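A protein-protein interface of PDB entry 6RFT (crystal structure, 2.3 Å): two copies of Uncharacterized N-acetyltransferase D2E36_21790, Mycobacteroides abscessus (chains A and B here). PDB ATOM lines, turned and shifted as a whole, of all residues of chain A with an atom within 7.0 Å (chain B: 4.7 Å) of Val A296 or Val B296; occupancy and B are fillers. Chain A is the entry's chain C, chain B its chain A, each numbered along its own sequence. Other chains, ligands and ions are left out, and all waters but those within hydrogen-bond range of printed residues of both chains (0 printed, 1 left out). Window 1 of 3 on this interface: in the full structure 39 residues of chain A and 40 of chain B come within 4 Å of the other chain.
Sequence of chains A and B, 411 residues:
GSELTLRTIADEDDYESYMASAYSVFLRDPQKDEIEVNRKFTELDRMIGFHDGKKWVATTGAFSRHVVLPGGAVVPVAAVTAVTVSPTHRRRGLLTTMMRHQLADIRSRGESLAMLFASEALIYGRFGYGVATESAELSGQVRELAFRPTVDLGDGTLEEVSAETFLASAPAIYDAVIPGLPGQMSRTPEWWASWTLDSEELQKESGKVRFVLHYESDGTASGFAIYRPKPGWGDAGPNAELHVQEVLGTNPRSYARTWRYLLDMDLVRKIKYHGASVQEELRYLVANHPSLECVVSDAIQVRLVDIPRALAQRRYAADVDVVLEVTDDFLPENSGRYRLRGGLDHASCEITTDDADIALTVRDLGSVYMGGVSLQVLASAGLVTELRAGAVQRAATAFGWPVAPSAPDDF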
ATOM      1  N   GLU A 134     -29.780   6.948  13.673  1.00  0.00           N
ATOM      2  CA  GLU A 134     -29.017   7.935  12.929  1.00  0.00           C
ATOM      3  C   GLU A 134     -28.283   8.857  13.891  1.00  0.00           C
ATOM      4  O   GLU A 134     -28.635   8.978  15.067  1.00  0.00           O
ATOM      5  CB  GLU A 134     -29.923   8.761  12.008  1.00  0.00           C
ATOM      6  CG  GLU A 134     -30.786   7.939  11.070  1.00  0.00           C
ATOM      7  CD  GLU A 134     -31.496   8.797  10.040  1.00  0.00           C
ATOM      8  OE1 GLU A 134     -30.894   9.073   8.981  1.00  0.00           O
ATOM      9  OE2 GLU A 134     -32.648   9.205  10.295  1.00  0.00           O
ATOM     10  N   SER A 135     -27.248   9.508  13.372  1.00  0.00           N
ATOM     11  CA  SER A 135     -26.497  10.506  14.114  1.00  0.00           C
ATOM     12  C   SER A 135     -26.354  11.748  13.251  1.00  0.00           C
ATOM     13  O   SER A 135     -26.406  11.677  12.019  1.00  0.00           O
ATOM     14  CB  SER A 135     -25.114   9.987  14.536  1.00  0.00           C
ATOM     15  OG  SER A 135     -24.282   9.774  13.410  1.00  0.00           O
ATOM     16  N   ALA A 136     -26.183  12.891  13.906  1.00  0.00           N
ATOM     17  CA  ALA A 136     -26.118  14.177  13.228  1.00  0.00           C
ATOM     18  C   ALA A 136     -24.780  14.836  13.521  1.00  0.00           C
ATOM     19  O   ALA A 136     -24.339  14.871  14.675  1.00  0.00           O
ATOM     20  CB  ALA A 136     -27.265  15.091  13.669  1.00  0.00           C
ATOM     21  N   GLU A 137     -24.138  15.354  12.477  1.00  0.00           N
ATOM     22  CA  GLU A 137     -22.937  16.166  12.628  1.00  0.00           C
ATOM     23  C   GLU A 137     -23.361  17.623  12.768  1.00  0.00           C
ATOM     24  O   GLU A 137     -23.883  18.221  11.823  1.00  0.00           O
ATOM     25  CB  GLU A 137     -21.993  15.970  11.444  1.00  0.00           C
ATOM     26  CG  GLU A 137     -20.686  16.734  11.569  1.00  0.00           C
ATOM     27  CD  GLU A 137     -19.725  16.437  10.436  1.00  0.00           C
ATOM     28  OE1 GLU A 137     -20.190  16.025   9.353  1.00  0.00           O
ATOM     29  OE2 GLU A 137     -18.507  16.641  10.620  1.00  0.00           O
ATOM     30  N   VAL A 278     -29.876  13.228  16.456  1.00  0.00           N
ATOM     31  CA  VAL A 278     -30.676  13.999  15.513  1.00  0.00           C
ATOM     32  C   VAL A 278     -31.628  14.945  16.233  1.00  0.00           C
ATOM     33  O   VAL A 278     -32.111  15.912  15.632  1.00  0.00           O
ATOM     34  CB  VAL A 278     -31.449  13.062  14.566  1.00  0.00           C
ATOM     35  CG1 VAL A 278     -30.481  12.231  13.737  1.00  0.00           C
ATOM     36  CG2 VAL A 278     -32.390  12.163  15.355  1.00  0.00           C
ATOM     37  N   ARG A 283     -29.502  21.667  19.711  1.00  0.00           N
ATOM     38  CA  ARG A 283     -30.155  22.223  18.529  1.00  0.00           C
ATOM     39  C   ARG A 283     -31.291  23.169  18.901  1.00  0.00           C
ATOM     40  O   ARG A 283     -31.547  24.143  18.182  1.00  0.00           O
ATOM     41  CB  ARG A 283     -30.677  21.090  17.644  1.00  0.00           C
ATOM     42  CG  ARG A 283     -29.624  20.047  17.300  1.00  0.00           C
ATOM     43  CD  ARG A 283     -30.134  19.019  16.301  1.00  0.00           C
ATOM     44  NE  ARG A 283     -30.452  19.613  15.005  1.00  0.00           N
ATOM     45  CZ  ARG A 283     -31.645  19.545  14.423  1.00  0.00           C
ATOM     46  NH1 ARG A 283     -32.640  18.901  15.016  1.00  0.00           N
ATOM     47  NH2 ARG A 283     -31.838  20.114  13.241  1.00  0.00           N
ATOM     48  N   HIS A 289     -31.759  28.778  15.082  1.00  0.00           N
ATOM     49  CA  HIS A 289     -31.725  27.377  14.662  1.00  0.00           C
ATOM     50  C   HIS A 289     -30.871  27.117  13.421  1.00  0.00           C
ATOM     51  O   HIS A 289     -30.086  26.155  13.441  1.00  0.00           O
ATOM     52  CB  HIS A 289     -33.179  26.920  14.474  1.00  0.00           C
ATOM     53  CG  HIS A 289     -33.365  25.435  14.463  1.00  0.00           C
ATOM     54  ND1 HIS A 289     -33.039  24.651  13.377  1.00  0.00           N
ATOM     55  CD2 HIS A 289     -33.884  24.596  15.390  1.00  0.00           C
ATOM     56  CE1 HIS A 289     -33.330  23.390  13.644  1.00  0.00           C
ATOM     57  NE2 HIS A 289     -33.844  23.329  14.860  1.00  0.00           N
ATOM     58  N   PRO A 290     -30.961  27.894  12.332  1.00  0.00           N
ATOM     59  CA  PRO A 290     -30.133  27.586  11.150  1.00  0.00           C
ATOM     60  C   PRO A 290     -28.639  27.768  11.370  1.00  0.00           C
ATOM     61  O   PRO A 290     -27.852  27.281  10.546  1.00  0.00           O
ATOM     62  CB  PRO A 290     -30.650  28.569  10.089  1.00  0.00           C
ATOM     63  CG  PRO A 290     -31.988  28.987  10.562  1.00  0.00           C
ATOM     64  CD  PRO A 290     -31.899  28.994  12.051  1.00  0.00           C
ATOM     65  N   LEU A 292     -26.789  26.315  13.400  1.00  0.00           N
ATOM     66  CA  LEU A 292     -26.197  25.029  13.753  1.00  0.00           C
ATOM     67  C   LEU A 292     -26.500  24.057  12.614  1.00  0.00           C
ATOM     68  O   LEU A 292     -27.562  23.432  12.576  1.00  0.00           O
ATOM     69  CB  LEU A 292     -26.738  24.525  15.091  1.00  0.00           C
ATOM     70  CG  LEU A 292     -26.107  23.251  15.654  1.00  0.00           C
ATOM     71  CD1 LEU A 292     -24.626  23.464  15.929  1.00  0.00           C
ATOM     72  CD2 LEU A 292     -26.832  22.806  16.915  1.00  0.00           C
ATOM     73  N   GLU A 293     -25.560  23.949  11.676  1.00  0.00           N
ATOM     74  CA  GLU A 293     -25.730  23.051  10.542  1.00  0.00           C
ATOM     75  C   GLU A 293     -25.854  21.610  11.024  1.00  0.00           C
ATOM     76  O   GLU A 293     -25.134  21.176  11.927  1.00  0.00           O
ATOM     77  CB  GLU A 293     -24.552  23.196   9.578  1.00  0.00           C
ATOM     78  CG  GLU A 293     -24.763  22.548   8.219  1.00  0.00           C
ATOM     79  CD  GLU A 293     -23.531  22.631   7.340  1.00  0.00           C
ATOM     80  OE1 GLU A 293     -22.454  22.171   7.776  1.00  0.00           O
ATOM     81  OE2 GLU A 293     -23.638  23.161   6.214  1.00  0.00           O
ATOM     82  N   CYS A 294     -26.773  20.866  10.413  1.00  0.00           N
ATOM     83  CA  CYS A 294     -27.093  19.505  10.837  1.00  0.00           C
ATOM     84  C   CYS A 294     -27.088  18.580   9.628  1.00  0.00           C
ATOM     85  O   CYS A 294     -27.967  18.676   8.765  1.00  0.00           O
ATOM     86  CB  CYS A 294     -28.449  19.461  11.546  1.00  0.00           C
ATOM     87  SG  CYS A 294     -28.981  17.807  12.039  1.00  0.00           S
ATOM     88  N   VAL A 295     -26.104  17.687   9.566  1.00  0.00           N
ATOM     89  CA  VAL A 295     -26.003  16.684   8.510  1.00  0.00           C
ATOM     90  C   VAL A 295     -26.252  15.321   9.143  1.00  0.00           C
ATOM     91  O   VAL A 295     -25.547  14.925  10.079  1.00  0.00           O
ATOM     92  CB  VAL A 295     -24.636  16.730   7.809  1.00  0.00           C
ATOM     93  CG1 VAL A 295     -24.568  15.680   6.710  1.00  0.00           C
ATOM     94  CG2 VAL A 295     -24.378  18.119   7.243  1.00  0.00           C
ATOM     95  N   VAL A 296     -27.251  14.604   8.632  1.00  0.00           N
ATOM     96  CA  VAL A 296     -27.709  13.346   9.210  1.00  0.00           C
ATOM     97  C   VAL A 296     -27.268  12.197   8.313  1.00  0.00           C
ATOM     98  O   VAL A 296     -27.324  12.300   7.082  1.00  0.00           O
ATOM     99  CB  VAL A 296     -29.240  13.349   9.394  1.00  0.00           C
ATOM    100  CG1 VAL A 296     -29.711  12.061  10.053  1.00  0.00           C
ATOM    101  CG2 VAL A 296     -29.672  14.560  10.207  1.00  0.00           C
ATOM    102  N   SER A 297     -26.838  11.098   8.933  1.00  0.00           N
ATOM    103  CA  SER A 297     -26.392   9.920   8.200  1.00  0.00           C
ATOM    104  C   SER A 297     -26.595   8.689   9.078  1.00  0.00           C
ATOM    105  O   SER A 297     -27.010   8.787  10.236  1.00  0.00           O
ATOM    106  CB  SER A 297     -24.932  10.063   7.759  1.00  0.00           C
ATOM    107  OG  SER A 297     -24.073  10.235   8.873  1.00  0.00           O
ATOM    108  N   ASP A 298     -26.295   7.522   8.510  1.00  0.00           N
ATOM    109  CA  ASP A 298     -26.472   6.263   9.222  1.00  0.00           C
ATOM    110  C   ASP A 298     -25.566   6.190  10.446  1.00  0.00           C
ATOM    111  O   ASP A 298     -24.466   6.749  10.471  1.00  0.00           O
ATOM    112  CB  ASP A 298     -26.174   5.080   8.301  1.00  0.00           C
ATOM    113  CG  ASP A 298     -27.297   4.799   7.328  1.00  0.00           C
ATOM    114  OD1 ASP A 298     -28.361   5.447   7.435  1.00  0.00           O
ATOM    115  OD2 ASP A 298     -27.117   3.920   6.460  1.00  0.00           O
ATOM    116  N   GLU B 134     -39.261  20.912   9.971  1.00  0.00           N
ATOM    117  CA  GLU B 134     -37.949  20.936   9.346  1.00  0.00           C
ATOM    118  C   GLU B 134     -38.043  20.377   7.933  1.00  0.00           C
ATOM    119  O   GLU B 134     -38.970  19.636   7.594  1.00  0.00           O
ATOM    120  CB  GLU B 134     -36.935  20.119  10.156  1.00  0.00           C
ATOM    121  CG  GLU B 134     -36.841  20.500  11.623  1.00  0.00           C
ATOM    122  CD  GLU B 134     -35.691  19.805  12.325  1.00  0.00           C
ATOM    123  OE1 GLU B 134     -34.719  20.492  12.702  1.00  0.00           O
ATOM    124  OE2 GLU B 134     -35.757  18.568  12.490  1.00  0.00           O
ATOM    125  N   SER B 135     -37.067  20.742   7.105  1.00  0.00           N
ATOM    126  CA  SER B 135     -36.953  20.217   5.754  1.00  0.00           C
ATOM    127  C   SER B 135     -35.517  19.779   5.506  1.00  0.00           C
ATOM    128  O   SER B 135     -34.580  20.296   6.120  1.00  0.00           O
ATOM    129  CB  SER B 135     -37.377  21.251   4.701  1.00  0.00           C
ATOM    130  OG  SER B 135     -36.477  22.343   4.666  1.00  0.00           O
ATOM    131  N   ALA B 136     -35.352  18.825   4.595  1.00  0.00           N
ATOM    132  CA  ALA B 136     -34.051  18.241   4.301  1.00  0.00           C
ATOM    133  C   ALA B 136     -33.714  18.455   2.833  1.00  0.00           C
ATOM    134  O   ALA B 136     -34.557  18.228   1.959  1.00  0.00           O
ATOM    135  CB  ALA B 136     -34.031  16.748   4.636  1.00  0.00           C
ATOM    136  N   VAL B 278     -37.884  15.496   6.062  1.00  0.00           N
ATOM    137  CA  VAL B 278     -36.811  14.848   6.807  1.00  0.00           C
ATOM    138  C   VAL B 278     -37.001  13.340   6.832  1.00  0.00           C
ATOM    139  O   VAL B 278     -36.045  12.597   7.078  1.00  0.00           O
ATOM    140  CB  VAL B 278     -36.722  15.418   8.238  1.00  0.00           C
ATOM    141  CG1 VAL B 278     -36.389  16.902   8.201  1.00  0.00           C
ATOM    142  CG2 VAL B 278     -38.020  15.174   8.991  1.00  0.00           C
ATOM    143  N   ARG B 283     -35.336   8.511   0.911  1.00  0.00           N
ATOM    144  CA  ARG B 283     -34.204   8.204   1.781  1.00  0.00           C
ATOM    145  C   ARG B 283     -34.152   6.725   2.140  1.00  0.00           C
ATOM    146  O   ARG B 283     -33.063   6.165   2.313  1.00  0.00           O
ATOM    147  CB  ARG B 283     -34.276   9.053   3.051  1.00  0.00           C
ATOM    148  CG  ARG B 283     -34.404  10.547   2.793  1.00  0.00           C
ATOM    149  CD  ARG B 283     -34.329  11.354   4.081  1.00  0.00           C
ATOM    150  NE  ARG B 283     -33.036  11.220   4.746  1.00  0.00           N
ATOM    151  CZ  ARG B 283     -32.876  10.777   5.990  1.00  0.00           C
ATOM    152  NH1 ARG B 283     -33.931  10.429   6.713  1.00  0.00           N
ATOM    153  NH2 ARG B 283     -31.661  10.689   6.513  1.00  0.00           N
ATOM    154  N   CYS B 294     -28.081  14.282   3.539  1.00  0.00           N
ATOM    155  CA  CYS B 294     -29.280  14.849   4.151  1.00  0.00           C
ATOM    156  C   CYS B 294     -28.875  15.982   5.084  1.00  0.00           C
ATOM    157  O   CYS B 294     -28.270  15.740   6.134  1.00  0.00           O
ATOM    158  CB  CYS B 294     -30.069  13.779   4.906  1.00  0.00           C
ATOM    159  SG  CYS B 294     -31.530  14.401   5.765  1.00  0.00           S
ATOM    160  N   VAL B 295     -29.204  17.214   4.704  1.00  0.00           N
ATOM    161  CA  VAL B 295     -28.943  18.400   5.514  1.00  0.00           C
ATOM    162  C   VAL B 295     -30.285  18.952   5.980  1.00  0.00           C
ATOM    163  O   VAL B 295     -31.151  19.270   5.156  1.00  0.00           O
ATOM    164  CB  VAL B 295     -28.152  19.458   4.731  1.00  0.00           C
ATOM    165  CG1 VAL B 295     -27.881  20.674   5.603  1.00  0.00           C
ATOM    166  CG2 VAL B 295     -26.851  18.870   4.204  1.00  0.00           C
ATOM    167  N   VAL B 296     -30.452  19.081   7.294  1.00  0.00           N
ATOM    168  CA  VAL B 296     -31.720  19.472   7.901  1.00  0.00           C
ATOM    169  C   VAL B 296     -31.610  20.909   8.398  1.00  0.00           C
ATOM    170  O   VAL B 296     -30.584  21.304   8.962  1.00  0.00           O
ATOM    171  CB  VAL B 296     -32.104  18.517   9.049  1.00  0.00           C
ATOM    172  CG1 VAL B 296     -33.454  18.898   9.641  1.00  0.00           C
ATOM    173  CG2 VAL B 296     -32.124  17.080   8.552  1.00  0.00           C
ATOM    174  N   SER B 297     -32.675  21.683   8.195  1.00  0.00           N
ATOM    175  CA  SER B 297     -32.712  23.081   8.605  1.00  0.00           C
ATOM    176  C   SER B 297     -34.163  23.488   8.839  1.00  0.00           C
ATOM    177  O   SER B 297     -35.092  22.697   8.645  1.00  0.00           O
ATOM    178  CB  SER B 297     -32.041  23.982   7.565  1.00  0.00           C
ATOM    179  OG  SER B 297     -32.688  23.880   6.308  1.00  0.00           O
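The backbone NH of Val A296 sits at hydrogen-bond distance from the backbone carbonyl oxygen of Cys B294 (2.9 Å).
NH2 of Arg B283 is in salt-bridge range of OE1 of Glu A134 (3.0 Å).
The side-chain carboxylate of Glu B134 lies within salt-bridge range of the guanidinium group of Arg A283 (3.0 Å).
The backbone NH of Val B296 sits at hydrogen-bond distance from the backbone carbonyl oxygen of Cys A294 (2.9 Å).
NE of Arg A283 lies within hydrogen-bond range of SG of Cys A294.
The backbone NH (N) of Glu A137 lies within hydrogen-bond range of the backbone carbonyl oxygen (O) of Val A295 (2.8 Å).
O of Val B278 is in hydrogen-bond range of NH1 of Arg B283, at 3.0 Å.
The backbone carbonyl oxygen of Val A278 lies within hydrogen-bond range of the guanidinium group of Arg A283 (3.1 Å).
The guanidinium group (NE) of Arg B283 lies within hydrogen-bond range of the side-chain sulfur (SG) of Cys B294.
Among the printed residues, pairs that only touch across the chains: His A289 with Glu B134 (3.3 Å), Cys A294 with Val B295 (3.4 Å), Val A295 with Cys B294 (3.4 Å), Val A296 with Val B296 (3.9 Å), Cys A294 with Cys B294 (3.95 Å) and Val A295 with Val B295 (3.99 Å).
Of the printed residues of chain B, Glu A134 touches Arg B283.
Printed residues of chain B within 4 Å of Cys A294: Cys B294 (3.95 Å), Val B295 (3.4 Å) and Val B296 (2.9 Å).
Val A296 touches just these residues of chain B: Cys B294 (2.9 Å) and Val B296 (3.9 Å).
Printed residues of chain A within 4 Å of Glu B134: Arg A283 and His A289.
Of the printed residues of chain A, Arg B283 touches Glu A134.
Of the printed residues of chain A, Val B295 touches Cys A294 and Val A295.
The nearest printed residue of chain A that does not touch Arg B283 is Val A296 (4.3 Å).
Of the 15 printed residues of chain A, 6 touch a printed residue of chain B.
Printed residues of chain A that touch a printed residue of chain B: Glu A134, Arg A283, His A289, Cys A294, Val A295 and Val A296.
Of the 9 printed residues of chain B, 5 touch a printed residue of chain A.
Among the printed residues, 10 pairs touch across the chains.
Among the printed residues, Asp or Glu carboxylates within 4 Å of a Lys or Arg side-chain nitrogen of the other chain: Glu A134 with Arg B283 (3.0 Å) and Arg A283 with Glu B134 (3.0 Å).
Cys A294 touches Val B295, and with the chains exchanged Val A295 touches Cys B294.
Cys A294 touches Val B296, and with the chains exchanged Val A296 touches Cys B294.
Val A295 touches its own counterpart, Val B295.
Val B296 touches its own counterpart, Val A296.
9 positions are printed for both chains.
Of the 10 pairs that touch across the chains among the printed residues, 9 have their exchanged pair printed and touching as well.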
